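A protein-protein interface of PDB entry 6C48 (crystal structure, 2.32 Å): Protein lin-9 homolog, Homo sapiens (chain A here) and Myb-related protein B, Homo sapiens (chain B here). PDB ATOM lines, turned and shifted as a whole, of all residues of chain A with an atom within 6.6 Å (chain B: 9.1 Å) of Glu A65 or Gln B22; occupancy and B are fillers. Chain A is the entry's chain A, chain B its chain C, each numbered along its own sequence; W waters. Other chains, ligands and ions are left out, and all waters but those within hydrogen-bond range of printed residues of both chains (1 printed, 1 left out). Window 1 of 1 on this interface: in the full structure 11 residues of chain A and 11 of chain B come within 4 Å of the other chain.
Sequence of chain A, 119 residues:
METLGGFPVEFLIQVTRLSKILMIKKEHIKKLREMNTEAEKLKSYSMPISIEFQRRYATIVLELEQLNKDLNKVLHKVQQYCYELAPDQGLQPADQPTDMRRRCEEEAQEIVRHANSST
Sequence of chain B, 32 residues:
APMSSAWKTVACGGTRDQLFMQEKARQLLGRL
Of the printed residues of chain B, Val A61 touches Met B21, Gln B22 and Ala B25. Glu A65 touches just these residues of chain B: Gln B22 and Arg B26. Of the printed residues of chain A, Gly B13 touches Asn A68. Printed residues of chain A within 4 Å of Met B21: Val A61 (3.6 Å). Gln B22 touches just these residues of chain A: Val A61, Leu A62 and Glu A65. Printed residues of chain A within 4 Å of Ala B25: Val A61 (3.7 Å) and Leu A62 (3.7 Å). Printed residues of chain A within 4 Å of Arg B31: Leu A62 (3.8 Å). The nearest residue of chain B that does not touch Glu A65 is Gln B18 (5.2 Å).
Among the printed residues, merely in contact across the chains: Asn A68 with Cys B12, Glu A65 with Gln B22, Asn A68 with Gly B13, Val A61 with Met B21, Leu A62 with Leu B29, Val A61 with Gln B22, Leu A62 with Arg B26, Leu A62 with Gln B22, Leu A62 with Ala B25, Val A61 with Ala B25 and Leu A62 with Arg B31.
ND2 of Asn A68 is in hydrogen-bond range of O of Leu A64, at 3.3 Å. The side-chain amino group of Lys A69 is in salt-bridge range of the side-chain carboxylate of Glu A65 (3.1 Å). The backbone carbonyl oxygen (O) of Gly B13 lies close to the side-chain amide oxygen (OE1) of Gln B18, at 3.4 Å. The backbone carbonyl oxygen (O) of Arg B26 is in hydrogen-bond range of the backbone NH (N) of Arg B31 (2.9 Å).
Printed residues of chain B that touch a printed residue of chain A: Cys B12, Gly B13, Gln B18, Met B21, Gln B22, Ala B25, Arg B26, Leu B29 and Arg B31. Along chain B the printed residues that touch a printed residue of chain A span positions 12 to 31. Hydrophobic or aromatic side chains of chain A within 4 Å of the printed part of chain B: Val A61 and Leu A62. Among the printed residues, 13 pairs touch across the chains. Among the printed residues, Asp or Glu carboxylates within 4 Å of a Lys or Arg side-chain nitrogen of the other chain: Glu A65 with Arg B26 (3.3 Å).
Water W1 lies within hydrogen-bond range of the backbone carbonyl oxygen (O) of Gly B13 (2.4 Å), the side-chain amide nitrogen (NE2) of Gln B22 (2.6 Å) and the side-chain amide nitrogen (ND2) of Asn A68 (3.1 Å).
The side-chain carboxylate (OE2) of Glu A65 is in salt-bridge range of the guanidinium group (NH1) of Arg B26, 3.3 Å away. The side-chain amide nitrogen (ND2) of Asn A68 lies close to the side-chain amide nitrogen (NE2) of Gln B18, 3.3 Å away.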
ATOM      1  N   ILE A  60      -9.708 -22.001 -25.875  1.00  0.00           N
ATOM      2  CA  ILE A  60      -8.473 -21.819 -26.629  1.00  0.00           C
ATOM      3  C   ILE A  60      -7.264 -22.140 -25.770  1.00  0.00           C
ATOM      4  O   ILE A  60      -6.283 -22.711 -26.252  1.00  0.00           O
ATOM      5  CB  ILE A  60      -8.395 -20.401 -27.220  1.00  0.00           C
ATOM      6  CG1 ILE A  60      -9.592 -20.145 -28.138  1.00  0.00           C
ATOM      7  CG2 ILE A  60      -7.106 -20.210 -27.976  1.00  0.00           C
ATOM      8  CD1 ILE A  60      -9.740 -18.718 -28.555  1.00  0.00           C
ATOM      9  N   VAL A  61      -7.313 -21.788 -24.489  1.00  0.00           N
ATOM     10  CA  VAL A  61      -6.192 -22.066 -23.598  1.00  0.00           C
ATOM     11  C   VAL A  61      -5.968 -23.569 -23.474  1.00  0.00           C
ATOM     12  O   VAL A  61      -4.835 -24.056 -23.562  1.00  0.00           O
ATOM     13  CB  VAL A  61      -6.418 -21.408 -22.228  1.00  0.00           C
ATOM     14  CG1 VAL A  61      -5.467 -21.979 -21.237  1.00  0.00           C
ATOM     15  CG2 VAL A  61      -6.245 -19.868 -22.325  1.00  0.00           C
ATOM     16  N   LEU A  62      -7.043 -24.332 -23.250  1.00  0.00           N
ATOM     17  CA  LEU A  62      -6.870 -25.776 -23.117  1.00  0.00           C
ATOM     18  C   LEU A  62      -6.475 -26.430 -24.440  1.00  0.00           C
ATOM     19  O   LEU A  62      -5.729 -27.419 -24.430  1.00  0.00           O
ATOM     20  CB  LEU A  62      -8.140 -26.422 -22.567  1.00  0.00           C
ATOM     21  CG  LEU A  62      -8.563 -25.977 -21.166  1.00  0.00           C
ATOM     22  CD1 LEU A  62      -9.761 -26.779 -20.699  1.00  0.00           C
ATOM     23  CD2 LEU A  62      -7.407 -26.093 -20.185  1.00  0.00           C
ATOM     24  N   GLU A  63      -6.962 -25.910 -25.579  1.00  0.00           N
ATOM     25  CA  GLU A  63      -6.539 -26.452 -26.871  1.00  0.00           C
ATOM     26  C   GLU A  63      -5.060 -26.186 -27.107  1.00  0.00           C
ATOM     27  O   GLU A  63      -4.323 -27.083 -27.527  1.00  0.00           O
ATOM     28  CB  GLU A  63      -7.357 -25.851 -28.020  1.00  0.00           C
ATOM     29  CG  GLU A  63      -8.800 -26.261 -28.010  1.00  0.00           C
ATOM     30  CD  GLU A  63      -9.591 -25.665 -29.155  1.00  0.00           C
ATOM     31  OE1 GLU A  63      -9.060 -24.770 -29.845  1.00  0.00           O
ATOM     32  OE2 GLU A  63     -10.759 -26.069 -29.344  1.00  0.00           O
ATOM     33  N   LEU A  64      -4.602 -24.972 -26.794  1.00  0.00           N
ATOM     34  CA  LEU A  64      -3.177 -24.692 -26.882  1.00  0.00           C
ATOM     35  C   LEU A  64      -2.375 -25.659 -26.018  1.00  0.00           C
ATOM     36  O   LEU A  64      -1.313 -26.138 -26.435  1.00  0.00           O
ATOM     37  CB  LEU A  64      -2.905 -23.257 -26.454  1.00  0.00           C
ATOM     38  CG  LEU A  64      -3.082 -22.145 -27.484  1.00  0.00           C
ATOM     39  CD1 LEU A  64      -2.975 -20.783 -26.805  1.00  0.00           C
ATOM     40  CD2 LEU A  64      -2.068 -22.287 -28.623  1.00  0.00           C
ATOM     41  N   GLU A  65      -2.892 -25.991 -24.830  1.00  0.00           N
ATOM     42  CA  GLU A  65      -2.177 -26.900 -23.947  1.00  0.00           C
ATOM     43  C   GLU A  65      -1.921 -28.234 -24.635  1.00  0.00           C
ATOM     44  O   GLU A  65      -0.830 -28.799 -24.532  1.00  0.00           O
ATOM     45  CB  GLU A  65      -2.969 -27.128 -22.660  1.00  0.00           C
ATOM     46  CG  GLU A  65      -2.186 -27.900 -21.620  1.00  0.00           C
ATOM     47  CD  GLU A  65      -3.023 -28.338 -20.433  1.00  0.00           C
ATOM     48  OE1 GLU A  65      -2.643 -29.331 -19.775  1.00  0.00           O
ATOM     49  OE2 GLU A  65      -4.053 -27.689 -20.146  1.00  0.00           O
ATOM     50  N   GLN A  66      -2.922 -28.749 -25.344  1.00  0.00           N
ATOM     51  CA  GLN A  66      -2.761 -30.018 -26.037  1.00  0.00           C
ATOM     52  C   GLN A  66      -1.823 -29.874 -27.226  1.00  0.00           C
ATOM     53  O   GLN A  66      -0.918 -30.696 -27.407  1.00  0.00           O
ATOM     54  CB  GLN A  66      -4.122 -30.537 -26.492  1.00  0.00           C
ATOM     55  CG  GLN A  66      -4.050 -31.825 -27.300  1.00  0.00           C
ATOM     56  CD  GLN A  66      -3.563 -32.990 -26.459  1.00  0.00           C
ATOM     57  OE1 GLN A  66      -2.685 -33.761 -26.873  1.00  0.00           O
ATOM     58  NE2 GLN A  66      -4.116 -33.108 -25.255  1.00  0.00           N
ATOM     59  N   LEU A  67      -2.012 -28.820 -28.040  1.00  0.00           N
ATOM     60  CA  LEU A  67      -1.121 -28.599 -29.175  1.00  0.00           C
ATOM     61  C   LEU A  67       0.329 -28.562 -28.718  1.00  0.00           C
ATOM     62  O   LEU A  67       1.208 -29.138 -29.370  1.00  0.00           O
ATOM     63  CB  LEU A  67      -1.484 -27.313 -29.913  1.00  0.00           C
ATOM     64  CG  LEU A  67      -2.692 -27.409 -30.844  1.00  0.00           C
ATOM     65  CD1 LEU A  67      -3.367 -26.052 -31.045  1.00  0.00           C
ATOM     66  CD2 LEU A  67      -2.340 -28.045 -32.186  1.00  0.00           C
ATOM     67  N   ASN A  68       0.585 -27.920 -27.573  1.00  0.00           N
ATOM     68  CA  ASN A  68       1.939 -27.814 -27.038  1.00  0.00           C
ATOM     69  C   ASN A  68       2.471 -29.161 -26.580  1.00  0.00           C
ATOM     70  O   ASN A  68       3.675 -29.414 -26.694  1.00  0.00           O
ATOM     71  CB  ASN A  68       1.975 -26.825 -25.874  1.00  0.00           C
ATOM     72  CG  ASN A  68       2.053 -25.403 -26.345  1.00  0.00           C
ATOM     73  OD1 ASN A  68       2.652 -25.121 -27.380  1.00  0.00           O
ATOM     74  ND2 ASN A  68       1.428 -24.496 -25.610  1.00  0.00           N
ATOM     75  N   LYS A  69       1.600 -30.027 -26.047  1.00  0.00           N
ATOM     76  CA  LYS A  69       2.039 -31.377 -25.724  1.00  0.00           C
ATOM     77  C   LYS A  69       2.410 -32.140 -26.984  1.00  0.00           C
ATOM     78  O   LYS A  69       3.416 -32.855 -27.001  1.00  0.00           O
ATOM     79  CB  LYS A  69       0.970 -32.103 -24.922  1.00  0.00           C
ATOM     80  CG  LYS A  69       0.953 -31.636 -23.474  1.00  0.00           C
ATOM     81  CD  LYS A  69       0.076 -32.498 -22.610  1.00  0.00           C
ATOM     82  CE  LYS A  69      -1.246 -31.827 -22.361  1.00  0.00           C
ATOM     83  NZ  LYS A  69      -1.743 -32.047 -20.968  1.00  0.00           N
ATOM     84  N   ASP A  70       1.625 -31.981 -28.056  1.00  0.00           N
ATOM     85  CA  ASP A  70       1.973 -32.601 -29.330  1.00  0.00           C
ATOM     86  C   ASP A  70       3.209 -31.957 -29.953  1.00  0.00           C
ATOM     87  O   ASP A  70       4.071 -32.657 -30.491  1.00  0.00           O
ATOM     88  CB  ASP A  70       0.794 -32.512 -30.291  1.00  0.00           C
ATOM     89  CG  ASP A  70      -0.434 -33.159 -29.743  1.00  0.00           C
ATOM     90  OD1 ASP A  70      -1.549 -32.796 -30.187  1.00  0.00           O
ATOM     91  OD2 ASP A  70      -0.281 -34.038 -28.865  1.00  0.00           O
ATOM     92  N   CYS B  12       7.209 -24.503 -26.492  1.00  0.00           N
ATOM     93  CA  CYS B  12       6.096 -25.389 -26.162  1.00  0.00           C
ATOM     94  C   CYS B  12       5.221 -24.839 -25.042  1.00  0.00           C
ATOM     95  O   CYS B  12       4.603 -25.608 -24.302  1.00  0.00           O
ATOM     96  CB  CYS B  12       6.591 -26.788 -25.785  1.00  0.00           C
ATOM     97  SG  CYS B  12       7.579 -27.632 -27.031  1.00  0.00           S
ATOM     98  N   GLY B  13       5.112 -23.515 -24.943  1.00  0.00           N
ATOM     99  CA  GLY B  13       4.133 -22.924 -24.058  1.00  0.00           C
ATOM    100  C   GLY B  13       4.222 -23.376 -22.616  1.00  0.00           C
ATOM    101  O   GLY B  13       3.214 -23.766 -22.023  1.00  0.00           O
ATOM    102  N   GLY B  14       5.423 -23.345 -22.042  1.00  0.00           N
ATOM    103  CA  GLY B  14       5.625 -23.763 -20.670  1.00  0.00           C
ATOM    104  C   GLY B  14       5.903 -22.670 -19.659  1.00  0.00           C
ATOM    105  O   GLY B  14       6.316 -22.985 -18.543  1.00  0.00           O
ATOM    106  N   THR B  15       5.716 -21.395 -20.004  1.00  0.00           N
ATOM    107  CA  THR B  15       6.006 -20.330 -19.048  1.00  0.00           C
ATOM    108  C   THR B  15       4.998 -20.310 -17.903  1.00  0.00           C
ATOM    109  O   THR B  15       3.877 -20.812 -18.013  1.00  0.00           O
ATOM    110  CB  THR B  15       6.011 -18.964 -19.720  1.00  0.00           C
ATOM    111  OG1 THR B  15       4.692 -18.658 -20.191  1.00  0.00           O
ATOM    112  CG2 THR B  15       6.999 -18.979 -20.874  1.00  0.00           C
ATOM    113  N   ARG B  16       5.422 -19.680 -16.800  1.00  0.00           N
ATOM    114  CA  ARG B  16       4.687 -19.727 -15.531  1.00  0.00           C
ATOM    115  C   ARG B  16       3.261 -19.192 -15.669  1.00  0.00           C
ATOM    116  O   ARG B  16       2.322 -19.771 -15.109  1.00  0.00           O
ATOM    117  CB  ARG B  16       5.482 -18.955 -14.466  1.00  0.00           C
ATOM    118  CG  ARG B  16       4.669 -18.246 -13.417  1.00  0.00           C
ATOM    119  CD  ARG B  16       5.500 -17.219 -12.607  1.00  0.00           C
ATOM    120  NE  ARG B  16       4.611 -16.299 -11.888  1.00  0.00           N
ATOM    121  CZ  ARG B  16       4.988 -15.418 -10.964  1.00  0.00           C
ATOM    122  NH1 ARG B  16       6.264 -15.307 -10.617  1.00  0.00           N
ATOM    123  NH2 ARG B  16       4.076 -14.637 -10.381  1.00  0.00           N
ATOM    124  N   ASP B  17       3.066 -18.096 -16.413  1.00  0.00           N
ATOM    125  CA  ASP B  17       1.707 -17.576 -16.569  1.00  0.00           C
ATOM    126  C   ASP B  17       0.848 -18.468 -17.462  1.00  0.00           C
ATOM    127  O   ASP B  17      -0.371 -18.535 -17.266  1.00  0.00           O
ATOM    128  CB  ASP B  17       1.727 -16.161 -17.135  1.00  0.00           C
ATOM    129  CG  ASP B  17       2.324 -15.158 -16.177  1.00  0.00           C
ATOM    130  OD1 ASP B  17       2.298 -15.401 -14.944  1.00  0.00           O
ATOM    131  OD2 ASP B  17       2.845 -14.138 -16.675  1.00  0.00           O
ATOM    132  N   GLN B  18       1.449 -19.153 -18.444  1.00  0.00           N
ATOM    133  CA  GLN B  18       0.651 -20.043 -19.282  1.00  0.00           C
ATOM    134  C   GLN B  18       0.149 -21.236 -18.485  1.00  0.00           C
ATOM    135  O   GLN B  18      -1.024 -21.611 -18.604  1.00  0.00           O
ATOM    136  CB  GLN B  18       1.442 -20.524 -20.499  1.00  0.00           C
ATOM    137  CG  GLN B  18       0.689 -21.543 -21.366  1.00  0.00           C
ATOM    138  CD  GLN B  18       1.045 -21.437 -22.843  1.00  0.00           C
ATOM    139  OE1 GLN B  18       2.031 -20.796 -23.215  1.00  0.00           O
ATOM    140  NE2 GLN B  18       0.241 -22.055 -23.687  1.00  0.00           N
ATOM    141  N   LEU B  19       1.015 -21.834 -17.656  1.00  0.00           N
ATOM    142  CA  LEU B  19       0.579 -22.923 -16.783  1.00  0.00           C
ATOM    143  C   LEU B  19      -0.494 -22.436 -15.815  1.00  0.00           C
ATOM    144  O   LEU B  19      -1.439 -23.168 -15.498  1.00  0.00           O
ATOM    145  CB  LEU B  19       1.772 -23.506 -16.020  1.00  0.00           C
ATOM    146  CG  LEU B  19       2.939 -24.115 -16.829  1.00  0.00           C
ATOM    147  CD1 LEU B  19       4.133 -24.490 -15.921  1.00  0.00           C
ATOM    148  CD2 LEU B  19       2.501 -25.317 -17.656  1.00  0.00           C
ATOM    149  N   PHE B  20      -0.374 -21.191 -15.360  1.00  0.00           N
ATOM    150  CA  PHE B  20      -1.403 -20.602 -14.518  1.00  0.00           C
ATOM    151  C   PHE B  20      -2.718 -20.493 -15.274  1.00  0.00           C
ATOM    152  O   PHE B  20      -3.762 -20.950 -14.798  1.00  0.00           O
ATOM    153  CB  PHE B  20      -0.932 -19.232 -14.026  1.00  0.00           C
ATOM    154  CG  PHE B  20      -1.949 -18.489 -13.241  1.00  0.00           C
ATOM    155  CD1 PHE B  20      -2.822 -17.621 -13.864  1.00  0.00           C
ATOM    156  CD2 PHE B  20      -2.029 -18.646 -11.869  1.00  0.00           C
ATOM    157  CE1 PHE B  20      -3.783 -16.933 -13.134  1.00  0.00           C
ATOM    158  CE2 PHE B  20      -2.982 -17.954 -11.125  1.00  0.00           C
ATOM    159  CZ  PHE B  20      -3.859 -17.103 -11.764  1.00  0.00           C
ATOM    160  N   MET B  21      -2.686 -19.905 -16.462  1.00  0.00           N
ATOM    161  CA  MET B  21      -3.895 -19.734 -17.266  1.00  0.00           C
ATOM    162  C   MET B  21      -4.560 -21.062 -17.620  1.00  0.00           C
ATOM    163  O   MET B  21      -5.778 -21.134 -17.713  1.00  0.00           O
ATOM    164  CB  MET B  21      -3.573 -18.955 -18.538  1.00  0.00           C
ATOM    165  CG  MET B  21      -3.285 -17.500 -18.251  1.00  0.00           C
ATOM    166  SD  MET B  21      -4.795 -16.620 -17.339  1.00  0.00           S
ATOM    167  CE  MET B  21      -5.759 -15.933 -18.891  1.00  0.00           C
ATOM    168  N   GLN B  22      -3.751 -22.106 -17.806  1.00  0.00           N
ATOM    169  CA  GLN B  22      -4.303 -23.427 -18.097  1.00  0.00           C
ATOM    170  C   GLN B  22      -5.064 -23.959 -16.897  1.00  0.00           C
ATOM    171  O   GLN B  22      -6.108 -24.596 -17.051  1.00  0.00           O
ATOM    172  CB  GLN B  22      -3.188 -24.389 -18.510  1.00  0.00           C
ATOM    173  CG  GLN B  22      -2.605 -24.059 -19.872  1.00  0.00           C
ATOM    174  CD  GLN B  22      -1.364 -24.874 -20.243  1.00  0.00           C
ATOM    175  OE1 GLN B  22      -0.760 -25.562 -19.410  1.00  0.00           O
ATOM    176  NE2 GLN B  22      -0.977 -24.783 -21.507  1.00  0.00           N
ATOM    177  N   GLU B  23      -4.546 -23.691 -15.698  1.00  0.00           N
ATOM    178  CA  GLU B  23      -5.218 -24.063 -14.457  1.00  0.00           C
ATOM    179  C   GLU B  23      -6.551 -23.327 -14.307  1.00  0.00           C
ATOM    180  O   GLU B  23      -7.576 -23.938 -13.986  1.00  0.00           O
ATOM    181  CB  GLU B  23      -4.273 -23.754 -13.284  1.00  0.00           C
ATOM    182  CG  GLU B  23      -4.800 -23.996 -11.880  1.00  0.00           C
ATOM    183  CD  GLU B  23      -4.507 -22.794 -10.941  1.00  0.00           C
ATOM    184  OE1 GLU B  23      -5.066 -22.759  -9.805  1.00  0.00           O
ATOM    185  OE2 GLU B  23      -3.719 -21.881 -11.343  1.00  0.00           O
ATOM    186  N   LYS B  24      -6.565 -22.017 -14.563  1.00  0.00           N
ATOM    187  CA  LYS B  24      -7.813 -21.258 -14.500  1.00  0.00           C
ATOM    188  C   LYS B  24      -8.809 -21.739 -15.551  1.00  0.00           C
ATOM    189  O   LYS B  24     -10.020 -21.783 -15.298  1.00  0.00           O
ATOM    190  CB  LYS B  24      -7.525 -19.773 -14.698  1.00  0.00           C
ATOM    191  CG  LYS B  24      -6.714 -19.126 -13.617  1.00  0.00           C
ATOM    192  CD  LYS B  24      -7.523 -18.912 -12.347  1.00  0.00           C
ATOM    193  CE  LYS B  24      -6.691 -19.255 -11.115  1.00  0.00           C
ATOM    194  NZ  LYS B  24      -7.011 -18.419  -9.919  1.00  0.00           N
ATOM    195  N   ALA B  25      -8.321 -22.097 -16.742  1.00  0.00           N
ATOM    196  CA  ALA B  25      -9.224 -22.562 -17.789  1.00  0.00           C
ATOM    197  C   ALA B  25      -9.875 -23.883 -17.402  1.00  0.00           C
ATOM    198  O   ALA B  25     -11.087 -24.058 -17.568  1.00  0.00           O
ATOM    199  CB  ALA B  25      -8.476 -22.691 -19.118  1.00  0.00           C
ATOM    200  N   ARG B  26      -9.094 -24.807 -16.843  1.00  0.00           N
ATOM    201  CA  ARG B  26      -9.674 -26.049 -16.337  1.00  0.00           C
ATOM    202  C   ARG B  26     -10.745 -25.766 -15.294  1.00  0.00           C
ATOM    203  O   ARG B  26     -11.836 -26.337 -15.341  1.00  0.00           O
ATOM    204  CB  ARG B  26      -8.576 -26.949 -15.762  1.00  0.00           C
ATOM    205  CG  ARG B  26      -7.744 -27.632 -16.840  1.00  0.00           C
ATOM    206  CD  ARG B  26      -6.927 -28.765 -16.268  1.00  0.00           C
ATOM    207  NE  ARG B  26      -5.941 -28.310 -15.290  1.00  0.00           N
ATOM    208  CZ  ARG B  26      -4.727 -27.872 -15.600  1.00  0.00           C
ATOM    209  NH1 ARG B  26      -4.338 -27.827 -16.870  1.00  0.00           N
ATOM    210  NH2 ARG B  26      -3.901 -27.495 -14.636  1.00  0.00           N
ATOM    211  N   GLN B  27     -10.456 -24.865 -14.350  1.00  0.00           N
ATOM    212  CA  GLN B  27     -11.412 -24.565 -13.288  1.00  0.00           C
ATOM    213  C   GLN B  27     -12.670 -23.912 -13.834  1.00  0.00           C
ATOM    214  O   GLN B  27     -13.778 -24.213 -13.375  1.00  0.00           O
ATOM    215  CB  GLN B  27     -10.766 -23.671 -12.235  1.00  0.00           C
ATOM    216  CG  GLN B  27      -9.713 -24.402 -11.419  1.00  0.00           C
ATOM    217  CD  GLN B  27      -8.906 -23.472 -10.584  1.00  0.00           C
ATOM    218  OE1 GLN B  27      -9.144 -22.272 -10.584  1.00  0.00           O
ATOM    219  NE2 GLN B  27      -7.920 -24.006  -9.891  1.00  0.00           N
ATOM    220  N   LEU B  28     -12.518 -22.979 -14.784  1.00  0.00           N
ATOM    221  CA  LEU B  28     -13.680 -22.290 -15.340  1.00  0.00           C
ATOM    222  C   LEU B  28     -14.581 -23.244 -16.112  1.00  0.00           C
ATOM    223  O   LEU B  28     -15.802 -23.064 -16.125  1.00  0.00           O
ATOM    224  CB  LEU B  28     -13.243 -21.141 -16.248  1.00  0.00           C
ATOM    225  CG  LEU B  28     -14.441 -20.330 -16.759  1.00  0.00           C
ATOM    226  CD1 LEU B  28     -14.717 -19.118 -15.851  1.00  0.00           C
ATOM    227  CD2 LEU B  28     -14.255 -19.926 -18.213  1.00  0.00           C
ATOM    228  N   LEU B  29     -14.000 -24.245 -16.765  1.00  0.00           N
ATOM    229  CA  LEU B  29     -14.760 -25.210 -17.543  1.00  0.00           C
ATOM    230  C   LEU B  29     -15.158 -26.453 -16.750  1.00  0.00           C
ATOM    231  O   LEU B  29     -15.917 -27.277 -17.269  1.00  0.00           O
ATOM    232  CB  LEU B  29     -13.964 -25.614 -18.788  1.00  0.00           C
ATOM    233  CG  LEU B  29     -13.679 -24.523 -19.830  1.00  0.00           C
ATOM    234  CD1 LEU B  29     -12.982 -25.121 -21.035  1.00  0.00           C
ATOM    235  CD2 LEU B  29     -14.953 -23.806 -20.270  1.00  0.00           C
ATOM    236  N   GLY B  30     -14.693 -26.602 -15.515  1.00  0.00           N
ATOM    237  CA  GLY B  30     -14.995 -27.802 -14.755  1.00  0.00           C
ATOM    238  C   GLY B  30     -14.291 -29.059 -15.238  1.00  0.00           C
ATOM    239  O   GLY B  30     -14.899 -30.138 -15.233  1.00  0.00           O
ATOM    240  N   ARG B  31     -13.021 -28.952 -15.657  1.00  0.00           N
ATOM    241  CA  ARG B  31     -12.235 -30.088 -16.129  1.00  0.00           C
ATOM    242  C   ARG B  31     -11.053 -30.340 -15.200  1.00  0.00           C
ATOM    243  O   ARG B  31     -10.371 -29.401 -14.784  1.00  0.00           O
ATOM    244  CB  ARG B  31     -11.732 -29.873 -17.568  1.00  0.00           C
ATOM    245  CG  ARG B  31     -12.863 -29.674 -18.570  1.00  0.00           C
ATOM    246  CD  ARG B  31     -12.338 -29.537 -19.970  1.00  0.00           C
ATOM    247  NE  ARG B  31     -13.311 -28.965 -20.900  1.00  0.00           N
ATOM    248  CZ  ARG B  31     -13.086 -28.812 -22.205  1.00  0.00           C
ATOM    249  NH1 ARG B  31     -11.922 -29.201 -22.729  1.00  0.00           N
ATOM    250  NH2 ARG B  31     -14.014 -28.258 -22.983  1.00  0.00           N
ATOM    251  N   LEU B  32     -10.798 -31.617 -14.897  1.00  0.00           N
ATOM    252  CA  LEU B  32      -9.639 -32.010 -14.082  1.00  0.00           C
ATOM    253  C   LEU B  32      -8.305 -31.634 -14.721  1.00  0.00           C
ATOM    254  O   LEU B  32      -7.889 -32.249 -15.694  1.00  0.00           O
ATOM    255  CB  LEU B  32      -9.633 -33.522 -13.840  1.00  0.00           C
ATOM    256  CG  LEU B  32     -10.362 -34.191 -12.677  1.00  0.00           C
ATOM    257  CD1 LEU B  32      -9.893 -35.633 -12.569  1.00  0.00           C
ATOM    258  CD2 LEU B  32     -10.051 -33.435 -11.401  1.00  0.00           C
HETATM  259  O   HOH W   1       1.355 -25.217 -22.607  1.00  0.00           O
